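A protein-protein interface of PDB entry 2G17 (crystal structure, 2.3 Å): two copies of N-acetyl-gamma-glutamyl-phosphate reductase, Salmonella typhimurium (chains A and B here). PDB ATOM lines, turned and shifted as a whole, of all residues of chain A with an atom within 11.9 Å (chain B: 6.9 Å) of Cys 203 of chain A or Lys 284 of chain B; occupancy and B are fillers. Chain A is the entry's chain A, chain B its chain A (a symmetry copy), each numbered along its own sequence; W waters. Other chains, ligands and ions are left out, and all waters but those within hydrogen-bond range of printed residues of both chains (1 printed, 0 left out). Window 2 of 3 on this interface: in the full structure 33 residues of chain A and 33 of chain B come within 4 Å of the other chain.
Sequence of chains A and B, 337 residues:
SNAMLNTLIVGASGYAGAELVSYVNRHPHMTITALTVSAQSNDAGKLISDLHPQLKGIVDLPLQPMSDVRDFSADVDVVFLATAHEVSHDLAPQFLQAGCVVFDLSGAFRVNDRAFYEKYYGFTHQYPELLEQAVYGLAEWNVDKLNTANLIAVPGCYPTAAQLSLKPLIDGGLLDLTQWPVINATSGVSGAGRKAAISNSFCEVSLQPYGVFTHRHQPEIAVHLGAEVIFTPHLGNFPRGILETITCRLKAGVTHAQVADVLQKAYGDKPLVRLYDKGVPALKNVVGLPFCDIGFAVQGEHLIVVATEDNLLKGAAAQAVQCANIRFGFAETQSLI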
ATOM      1  N   VAL A 189      37.985  16.541 -15.523  1.00  0.00           N
ATOM      2  CA  VAL A 189      37.907  16.535 -16.987  1.00  0.00           C
ATOM      3  C   VAL A 189      39.181  16.946 -17.746  1.00  0.00           C
ATOM      4  O   VAL A 189      39.320  16.613 -18.936  1.00  0.00           O
ATOM      5  CB  VAL A 189      36.693  17.379 -17.479  1.00  0.00           C
ATOM      6  CG1 VAL A 189      36.376  17.035 -18.884  1.00  0.00           C
ATOM      7  CG2 VAL A 189      35.452  17.089 -16.598  1.00  0.00           C
ATOM      8  N   LYS A 195      40.478  19.825 -25.888  1.00  0.00           N
ATOM      9  CA  LYS A 195      39.896  19.342 -27.149  1.00  0.00           C
ATOM     10  C   LYS A 195      38.427  19.579 -27.090  1.00  0.00           C
ATOM     11  O   LYS A 195      37.794  19.463 -26.026  1.00  0.00           O
ATOM     12  CB  LYS A 195      40.139  17.850 -27.346  1.00  0.00           C
ATOM     13  CG  LYS A 195      39.238  16.964 -26.465  1.00  0.00           C
ATOM     14  CD  LYS A 195      39.907  15.619 -26.088  1.00  0.00           C
ATOM     15  CE  LYS A 195      38.921  14.452 -26.222  1.00  0.00           C
ATOM     16  NZ  LYS A 195      38.037  14.156 -25.040  1.00  0.00           N
ATOM     17  N   ALA A 196      37.893  19.963 -28.226  1.00  0.00           N
ATOM     18  CA  ALA A 196      36.483  20.109 -28.378  1.00  0.00           C
ATOM     19  C   ALA A 196      35.930  18.699 -28.692  1.00  0.00           C
ATOM     20  O   ALA A 196      36.057  18.206 -29.822  1.00  0.00           O
ATOM     21  CB  ALA A 196      36.210  21.089 -29.517  1.00  0.00           C
ATOM     22  N   ALA A 197      35.352  18.031 -27.695  1.00  0.00           N
ATOM     23  CA  ALA A 197      34.604  16.784 -27.960  1.00  0.00           C
ATOM     24  C   ALA A 197      33.302  16.818 -27.172  1.00  0.00           C
ATOM     25  O   ALA A 197      33.215  17.516 -26.157  1.00  0.00           O
ATOM     26  CB  ALA A 197      35.448  15.538 -27.596  1.00  0.00           C
ATOM     27  N   ILE A 198      32.299  16.077 -27.633  1.00  0.00           N
ATOM     28  CA  ILE A 198      31.010  16.000 -26.929  1.00  0.00           C
ATOM     29  C   ILE A 198      31.191  15.519 -25.471  1.00  0.00           C
ATOM     30  O   ILE A 198      30.663  16.139 -24.545  1.00  0.00           O
ATOM     31  CB  ILE A 198      29.933  15.139 -27.703  1.00  0.00           C
ATOM     32  CG1 ILE A 198      29.454  15.878 -28.964  1.00  0.00           C
ATOM     33  CG2 ILE A 198      28.708  14.853 -26.843  1.00  0.00           C
ATOM     34  CD1 ILE A 198      28.721  17.216 -28.704  1.00  0.00           C
ATOM     35  N   SER A 199      31.979  14.457 -25.285  1.00  0.00           N
ATOM     36  CA  SER A 199      32.089  13.806 -23.978  1.00  0.00           C
ATOM     37  C   SER A 199      32.796  14.643 -22.888  1.00  0.00           C
ATOM     38  O   SER A 199      32.542  14.425 -21.698  1.00  0.00           O
ATOM     39  CB  SER A 199      32.748  12.420 -24.107  1.00  0.00           C
ATOM     40  OG  SER A 199      34.118  12.553 -24.483  1.00  0.00           O
ATOM     41  N   ASN A 200      33.668  15.582 -23.266  1.00  0.00           N
ATOM     42  CA  ASN A 200      34.217  16.520 -22.258  1.00  0.00           C
ATOM     43  C   ASN A 200      33.566  17.934 -22.297  1.00  0.00           C
ATOM     44  O   ASN A 200      34.030  18.876 -21.630  1.00  0.00           O
ATOM     45  CB  ASN A 200      35.748  16.592 -22.315  1.00  0.00           C
ATOM     46  CG  ASN A 200      36.278  17.203 -23.629  1.00  0.00           C
ATOM     47  OD1 ASN A 200      35.594  17.200 -24.666  1.00  0.00           O
ATOM     48  ND2 ASN A 200      37.506  17.714 -23.584  1.00  0.00           N
ATOM     49  N   SER A 201      32.502  18.067 -23.087  1.00  0.00           N
ATOM     50  CA  SER A 201      31.734  19.311 -23.158  1.00  0.00           C
ATOM     51  C   SER A 201      31.062  19.528 -21.797  1.00  0.00           C
ATOM     52  O   SER A 201      30.699  18.553 -21.123  1.00  0.00           O
ATOM     53  CB  SER A 201      30.711  19.247 -24.297  1.00  0.00           C
ATOM     54  OG  SER A 201      30.039  20.469 -24.446  1.00  0.00           O
ATOM     55  N   PHE A 202      30.946  20.788 -21.369  1.00  0.00           N
ATOM     56  CA  PHE A 202      30.538  21.071 -19.982  1.00  0.00           C
ATOM     57  C   PHE A 202      29.280  20.312 -19.559  1.00  0.00           C
ATOM     58  O   PHE A 202      29.278  19.641 -18.523  1.00  0.00           O
ATOM     59  CB  PHE A 202      30.361  22.574 -19.691  1.00  0.00           C
ATOM     60  CG  PHE A 202      30.087  22.861 -18.231  1.00  0.00           C
ATOM     61  CD1 PHE A 202      31.142  23.185 -17.358  1.00  0.00           C
ATOM     62  CD2 PHE A 202      28.776  22.757 -17.710  1.00  0.00           C
ATOM     63  CE1 PHE A 202      30.897  23.419 -16.003  1.00  0.00           C
ATOM     64  CE2 PHE A 202      28.529  22.957 -16.358  1.00  0.00           C
ATOM     65  CZ  PHE A 202      29.581  23.283 -15.498  1.00  0.00           C
ATOM     66  N   CYS A 203      28.207  20.444 -20.343  1.00  0.00           N
ATOM     67  CA  CYS A 203      26.908  19.893 -19.939  1.00  0.00           C
ATOM     68  C   CYS A 203      26.850  18.363 -19.976  1.00  0.00           C
ATOM     69  O   CYS A 203      25.923  17.774 -19.445  1.00  0.00           O
ATOM     70  CB  CYS A 203      25.782  20.470 -20.780  1.00  0.00           C
ATOM     71  SG  CYS A 203      25.544  22.224 -20.448  1.00  0.00           S
ATOM     72  N   GLU A 204      27.828  17.751 -20.637  1.00  0.00           N
ATOM     73  CA  GLU A 204      27.878  16.306 -20.763  1.00  0.00           C
ATOM     74  C   GLU A 204      28.538  15.595 -19.566  1.00  0.00           C
ATOM     75  O   GLU A 204      28.500  14.376 -19.512  1.00  0.00           O
ATOM     76  CB  GLU A 204      28.553  15.915 -22.092  1.00  0.00           C
ATOM     77  CG  GLU A 204      27.793  16.456 -23.304  1.00  0.00           C
ATOM     78  CD  GLU A 204      26.392  15.875 -23.451  1.00  0.00           C
ATOM     79  OE1 GLU A 204      26.261  14.641 -23.433  1.00  0.00           O
ATOM     80  OE2 GLU A 204      25.415  16.640 -23.613  1.00  0.00           O
ATOM     81  N   VAL A 205      29.131  16.341 -18.624  1.00  0.00           N
ATOM     82  CA  VAL A 205      29.865  15.724 -17.504  1.00  0.00           C
ATOM     83  C   VAL A 205      29.071  15.753 -16.184  1.00  0.00           C
ATOM     84  O   VAL A 205      28.464  16.755 -15.829  1.00  0.00           O
ATOM     85  CB  VAL A 205      31.266  16.362 -17.295  1.00  0.00           C
ATOM     86  CG1 VAL A 205      32.089  15.554 -16.309  1.00  0.00           C
ATOM     87  CG2 VAL A 205      32.015  16.512 -18.644  1.00  0.00           C
ATOM     88  N   SER A 206      29.118  14.638 -15.453  1.00  0.00           N
ATOM     89  CA  SER A 206      28.390  14.479 -14.180  1.00  0.00           C
ATOM     90  C   SER A 206      29.250  13.499 -13.348  1.00  0.00           C
ATOM     91  O   SER A 206      30.206  13.905 -12.679  1.00  0.00           O
ATOM     92  CB  SER A 206      26.957  13.943 -14.426  1.00  0.00           C
ATOM     93  OG  SER A 206      26.955  12.750 -15.237  1.00  0.00           O
ATOM     94  N   LEU A 207      28.929  12.213 -13.425  1.00  0.00           N
ATOM     95  CA  LEU A 207      29.800  11.147 -12.942  1.00  0.00           C
ATOM     96  C   LEU A 207      29.395   9.927 -13.745  1.00  0.00           C
ATOM     97  O   LEU A 207      28.211   9.587 -13.797  1.00  0.00           O
ATOM     98  CB  LEU A 207      29.592  10.888 -11.412  1.00  0.00           C
ATOM     99  CG  LEU A 207      30.543   9.867 -10.745  1.00  0.00           C
ATOM    100  CD1 LEU A 207      32.005  10.189 -10.992  1.00  0.00           C
ATOM    101  CD2 LEU A 207      30.236   9.698  -9.232  1.00  0.00           C
ATOM    102  N   GLN A 208      30.374   9.285 -14.378  1.00  0.00           N
ATOM    103  CA  GLN A 208      30.121   8.050 -15.164  1.00  0.00           C
ATOM    104  C   GLN A 208      31.390   7.243 -15.272  1.00  0.00           C
ATOM    105  O   GLN A 208      32.430   7.823 -15.528  1.00  0.00           O
ATOM    106  CB  GLN A 208      29.699   8.371 -16.590  1.00  0.00           C
ATOM    107  CG  GLN A 208      29.170   7.167 -17.384  1.00  0.00           C
ATOM    108  CD  GLN A 208      28.755   7.572 -18.784  1.00  0.00           C
ATOM    109  OE1 GLN A 208      29.172   8.649 -19.263  1.00  0.00           O
ATOM    110  NE2 GLN A 208      27.928   6.734 -19.457  1.00  0.00           N
ATOM    111  N   PRO A 209      31.305   5.909 -15.036  1.00  0.00           N
ATOM    112  CA  PRO A 209      32.431   5.021 -15.344  1.00  0.00           C
ATOM    113  C   PRO A 209      32.622   4.963 -16.850  1.00  0.00           C
ATOM    114  O   PRO A 209      31.653   5.169 -17.596  1.00  0.00           O
ATOM    115  CB  PRO A 209      31.995   3.644 -14.790  1.00  0.00           C
ATOM    116  CG  PRO A 209      30.745   3.891 -14.003  1.00  0.00           C
ATOM    117  CD  PRO A 209      30.145   5.180 -14.476  1.00  0.00           C
ATOM    118  N   HIS A 234      36.437   6.881 -13.827  1.00  0.00           N
ATOM    119  CA  HIS A 234      35.154   7.607 -13.797  1.00  0.00           C
ATOM    120  C   HIS A 234      35.491   9.046 -14.103  1.00  0.00           C
ATOM    121  O   HIS A 234      36.483   9.562 -13.600  1.00  0.00           O
ATOM    122  CB  HIS A 234      34.486   7.584 -12.399  1.00  0.00           C
ATOM    123  CG  HIS A 234      34.145   6.222 -11.896  1.00  0.00           C
ATOM    124  ND1 HIS A 234      35.104   5.308 -11.524  1.00  0.00           N
ATOM    125  CD2 HIS A 234      32.947   5.623 -11.671  1.00  0.00           C
ATOM    126  CE1 HIS A 234      34.515   4.193 -11.115  1.00  0.00           C
ATOM    127  NE2 HIS A 234      33.207   4.361 -11.186  1.00  0.00           N
ATOM    128  N   LEU A 235      34.659   9.697 -14.917  1.00  0.00           N
ATOM    129  CA  LEU A 235      34.843  11.105 -15.221  1.00  0.00           C
ATOM    130  C   LEU A 235      33.914  11.871 -14.300  1.00  0.00           C
ATOM    131  O   LEU A 235      32.708  11.638 -14.321  1.00  0.00           O
ATOM    132  CB  LEU A 235      34.435  11.384 -16.676  1.00  0.00           C
ATOM    133  CG  LEU A 235      34.876  12.692 -17.323  1.00  0.00           C
ATOM    134  CD1 LEU A 235      36.435  12.810 -17.311  1.00  0.00           C
ATOM    135  CD2 LEU A 235      34.317  12.749 -18.738  1.00  0.00           C
ATOM    136  N   GLY A 236      34.483  12.758 -13.484  1.00  0.00           N
ATOM    137  CA  GLY A 236      33.702  13.583 -12.576  1.00  0.00           C
ATOM    138  C   GLY A 236      33.659  15.038 -13.042  1.00  0.00           C
ATOM    139  O   GLY A 236      34.517  15.473 -13.822  1.00  0.00           O
ATOM    140  N   ASN A 237      32.687  15.798 -12.542  1.00  0.00           N
ATOM    141  CA  ASN A 237      32.521  17.158 -12.998  1.00  0.00           C
ATOM    142  C   ASN A 237      33.283  18.162 -12.120  1.00  0.00           C
ATOM    143  O   ASN A 237      32.684  18.954 -11.402  1.00  0.00           O
ATOM    144  CB  ASN A 237      31.030  17.537 -13.138  1.00  0.00           C
ATOM    145  CG  ASN A 237      30.296  17.479 -11.816  1.00  0.00           C
ATOM    146  OD1 ASN A 237      30.618  16.633 -10.969  1.00  0.00           O
ATOM    147  ND2 ASN A 237      29.321  18.392 -11.612  1.00  0.00           N
ATOM    148  N   PHE A 238      34.604  18.112 -12.211  1.00  0.00           N
ATOM    149  CA  PHE A 238      35.474  19.088 -11.613  1.00  0.00           C
ATOM    150  C   PHE A 238      36.671  19.027 -12.585  1.00  0.00           C
ATOM    151  O   PHE A 238      36.817  18.040 -13.307  1.00  0.00           O
ATOM    152  CB  PHE A 238      35.811  18.747 -10.137  1.00  0.00           C
ATOM    153  CG  PHE A 238      36.300  17.317  -9.930  1.00  0.00           C
ATOM    154  CD1 PHE A 238      35.388  16.290  -9.621  1.00  0.00           C
ATOM    155  CD2 PHE A 238      37.652  17.001 -10.096  1.00  0.00           C
ATOM    156  CE1 PHE A 238      35.828  14.956  -9.457  1.00  0.00           C
ATOM    157  CE2 PHE A 238      38.109  15.687  -9.945  1.00  0.00           C
ATOM    158  CZ  PHE A 238      37.204  14.660  -9.625  1.00  0.00           C
ATOM    159  N   ARG B 240      23.110  16.521  -5.928  1.00  0.00           N
ATOM    160  CA  ARG B 240      22.113  15.461  -6.005  1.00  0.00           C
ATOM    161  C   ARG B 240      22.602  14.277  -6.824  1.00  0.00           C
ATOM    162  O   ARG B 240      23.286  14.452  -7.857  1.00  0.00           O
ATOM    163  CB  ARG B 240      20.817  15.986  -6.668  1.00  0.00           C
ATOM    164  CG  ARG B 240      20.126  17.192  -5.993  1.00  0.00           C
ATOM    165  CD  ARG B 240      18.968  16.819  -5.133  1.00  0.00           C
ATOM    166  NE  ARG B 240      17.870  16.114  -5.853  1.00  0.00           N
ATOM    167  CZ  ARG B 240      16.648  16.601  -6.099  1.00  0.00           C
ATOM    168  NH1 ARG B 240      16.287  17.828  -5.718  1.00  0.00           N
ATOM    169  NH2 ARG B 240      15.766  15.839  -6.718  1.00  0.00           N
ATOM    170  N   PRO B 281      25.199   3.691 -16.859  1.00  0.00           N
ATOM    171  CA  PRO B 281      24.622   5.025 -16.753  1.00  0.00           C
ATOM    172  C   PRO B 281      25.533   6.140 -16.229  1.00  0.00           C
ATOM    173  O   PRO B 281      26.477   5.890 -15.454  1.00  0.00           O
ATOM    174  CB  PRO B 281      23.423   4.822 -15.802  1.00  0.00           C
ATOM    175  CG  PRO B 281      23.775   3.586 -14.983  1.00  0.00           C
ATOM    176  CD  PRO B 281      24.578   2.719 -15.930  1.00  0.00           C
ATOM    177  N   ALA B 282      25.225   7.366 -16.676  1.00  0.00           N
ATOM    178  CA  ALA B 282      25.848   8.588 -16.194  1.00  0.00           C
ATOM    179  C   ALA B 282      24.890   9.195 -15.161  1.00  0.00           C
ATOM    180  O   ALA B 282      23.652   9.163 -15.313  1.00  0.00           O
ATOM    181  CB  ALA B 282      26.104   9.545 -17.350  1.00  0.00           C
ATOM    182  N   LEU B 283      25.449   9.707 -14.083  1.00  0.00           N
ATOM    183  CA  LEU B 283      24.631  10.184 -12.985  1.00  0.00           C
ATOM    184  C   LEU B 283      23.620  11.289 -13.366  1.00  0.00           C
ATOM    185  O   LEU B 283      22.496  11.271 -12.869  1.00  0.00           O
ATOM    186  CB  LEU B 283      25.531  10.639 -11.836  1.00  0.00           C
ATOM    187  CG  LEU B 283      24.851  11.062 -10.544  1.00  0.00           C
ATOM    188  CD1 LEU B 283      23.688  10.074 -10.174  1.00  0.00           C
ATOM    189  CD2 LEU B 283      25.884  11.109  -9.422  1.00  0.00           C
ATOM    190  N   LYS B 284      23.990  12.251 -14.220  1.00  0.00           N
ATOM    191  CA  LYS B 284      23.012  13.321 -14.523  1.00  0.00           C
ATOM    192  C   LYS B 284      21.697  12.855 -15.174  1.00  0.00           C
ATOM    193  O   LYS B 284      20.733  13.612 -15.193  1.00  0.00           O
ATOM    194  CB  LYS B 284      23.603  14.415 -15.413  1.00  0.00           C
ATOM    195  CG  LYS B 284      23.769  13.923 -16.821  1.00  0.00           C
ATOM    196  CD  LYS B 284      24.221  15.065 -17.730  1.00  0.00           C
ATOM    197  CE  LYS B 284      24.667  14.506 -19.046  1.00  0.00           C
ATOM    198  NZ  LYS B 284      23.456  14.328 -19.908  1.00  0.00           N
ATOM    199  N   ASN B 285      21.652  11.643 -15.726  1.00  0.00           N
ATOM    200  CA  ASN B 285      20.478  11.249 -16.480  1.00  0.00           C
ATOM    201  C   ASN B 285      19.348  10.732 -15.592  1.00  0.00           C
ATOM    202  O   ASN B 285      18.246  10.480 -16.062  1.00  0.00           O
ATOM    203  CB  ASN B 285      20.872  10.270 -17.573  1.00  0.00           C
ATOM    204  CG  ASN B 285      21.841  10.885 -18.522  1.00  0.00           C
ATOM    205  OD1 ASN B 285      21.686  12.039 -18.882  1.00  0.00           O
ATOM    206  ND2 ASN B 285      22.883  10.167 -18.878  1.00  0.00           N
ATOM    207  N   VAL B 286      19.618  10.593 -14.298  1.00  0.00           N
ATOM    208  CA  VAL B 286      18.571  10.237 -13.339  1.00  0.00           C
ATOM    209  C   VAL B 286      18.269  11.371 -12.335  1.00  0.00           C
ATOM    210  O   VAL B 286      17.266  11.327 -11.619  1.00  0.00           O
ATOM    211  CB  VAL B 286      18.938   8.865 -12.627  1.00  0.00           C
ATOM    212  CG1 VAL B 286      20.071   9.083 -11.604  1.00  0.00           C
ATOM    213  CG2 VAL B 286      17.669   8.199 -12.045  1.00  0.00           C
ATOM    214  N   VAL B 287      19.117  12.395 -12.274  1.00  0.00           N
ATOM    215  CA  VAL B 287      18.903  13.484 -11.317  1.00  0.00           C
ATOM    216  C   VAL B 287      17.557  14.187 -11.621  1.00  0.00           C
ATOM    217  O   VAL B 287      17.261  14.477 -12.802  1.00  0.00           O
ATOM    218  CB  VAL B 287      20.091  14.503 -11.305  1.00  0.00           C
ATOM    219  CG1 VAL B 287      19.703  15.848 -10.507  1.00  0.00           C
ATOM    220  CG2 VAL B 287      21.307  13.821 -10.707  1.00  0.00           C
ATOM    221  N   GLY B 288      16.734  14.409 -10.589  1.00  0.00           N
ATOM    222  CA  GLY B 288      15.385  14.995 -10.800  1.00  0.00           C
ATOM    223  C   GLY B 288      14.326  13.976 -11.212  1.00  0.00           C
ATOM    224  O   GLY B 288      13.154  14.337 -11.378  1.00  0.00           O
ATOM    225  N   LEU B 289      14.720  12.699 -11.337  1.00  0.00           N
ATOM    226  CA  LEU B 289      13.804  11.607 -11.751  1.00  0.00           C
ATOM    227  C   LEU B 289      13.718  10.536 -10.657  1.00  0.00           C
ATOM    228  O   LEU B 289      14.643  10.421  -9.845  1.00  0.00           O
ATOM    229  CB  LEU B 289      14.279  10.968 -13.076  1.00  0.00           C
ATOM    230  CG  LEU B 289      14.291  11.918 -14.270  1.00  0.00           C
ATOM    231  CD1 LEU B 289      15.009  11.262 -15.457  1.00  0.00           C
ATOM    232  CD2 LEU B 289      12.843  12.389 -14.657  1.00  0.00           C
ATOM    233  N   THR B 308      22.622   4.032 -10.583  1.00  0.00           N
ATOM    234  CA  THR B 308      22.463   5.451 -10.217  1.00  0.00           C
ATOM    235  C   THR B 308      21.039   5.690  -9.719  1.00  0.00           C
ATOM    236  O   THR B 308      20.123   4.948 -10.057  1.00  0.00           O
ATOM    237  CB  THR B 308      22.688   6.405 -11.403  1.00  0.00           C
ATOM    238  OG1 THR B 308      21.814   6.004 -12.456  1.00  0.00           O
ATOM    239  CG2 THR B 308      24.117   6.359 -11.923  1.00  0.00           C
HETATM  240  O   HOH W   1      24.251  13.049 -22.405  1.00  0.00           O
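O of Gln 208 of chain A lies within hydrogen-bond range of N of Leu 235 of chain A. The side-chain amino group (NZ) of Lys 284 of chain B lies within hydrogen-bond range of the side-chain amide oxygen (OD1) of Asn 285 of chain B (3.1 Å). The backbone carbonyl oxygen (O) of Ser 206 of chain A is in hydrogen-bond range of the backbone NH (N) of Asn 237 of chain A.
Of chain B, only Lys 284 comes within 4 Å of Cys 203 of chain A. Printed residues of chain B within 4 Å of Leu 207 of chain A: Ala 282 (3.5 Å) and Leu 283 (2.8 Å). Of the printed residues of chain A, Pro 281 of chain B touches Gln 208 (3.6 Å) and Pro 209 (3.9 Å). Leu 283 of chain B touches just these residues of chain A: Ser 206 (3.6 Å) and Leu 207 (2.8 Å). Of chain A, only Cys 203, Glu 204 and Ser 206 come within 4 Å of Lys 284 of chain B. No residue of chain A comes within 4 Å of Val 286 of chain B. No residue of chain A comes within 4 Å of Val 287 of chain B. The nearest printed residue of chain B that does not touch Cys 203 of chain A is Asn 285 of chain B (7.2 Å).
The side-chain hydroxyl (OG) of Ser 206 of chain A sits at hydrogen-bond distance from the backbone NH (N) of Lys 284 of chain B (3.2 Å). The backbone NH (N) of Leu 283 of chain B is in hydrogen-bond range of the backbone carbonyl oxygen (O) of Leu 207 of chain A, 2.8 Å away.
Cys 203 of chain A touches Lys 284 of chain B. Glu 204 of chain A touches Lys 284 of chain B. Ser 206 of chain A touches Ala 282 of chain B. OG of Ser 206 of chain A touches N of Leu 283 of chain B, 3.6 Å away. Leu 207 of chain A touches Ala 282 of chain B. CG of Gln 208 of chain A touches O of Pro 281 of chain B (3.6 Å). CB of Ala 282 of chain B touches CD of Gln 208 of chain A (3.6 Å). Pro 281 of chain B touches Pro 209 of chain A.
Of the 21 printed residues of chain A, 6 touch a printed residue of chain B. Hydrophobic or aromatic side chains of chain A that line the printed part of chain B: Pro 209. Along chain A the printed residues that touch a printed residue of chain B span positions 203 to 209. Hydrophobic or aromatic side chains of chain B that line the printed part of chain A: Ala 282 and Leu 283.
No position is printed for both chains. Of the 10 pairs that touch across the chains among the printed residues, none has its exchanged pair printed and touching as well.
Water W1 lies within hydrogen-bond range of OE1 of Glu 204 of chain A and NZ of Lys 284 of chain B.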
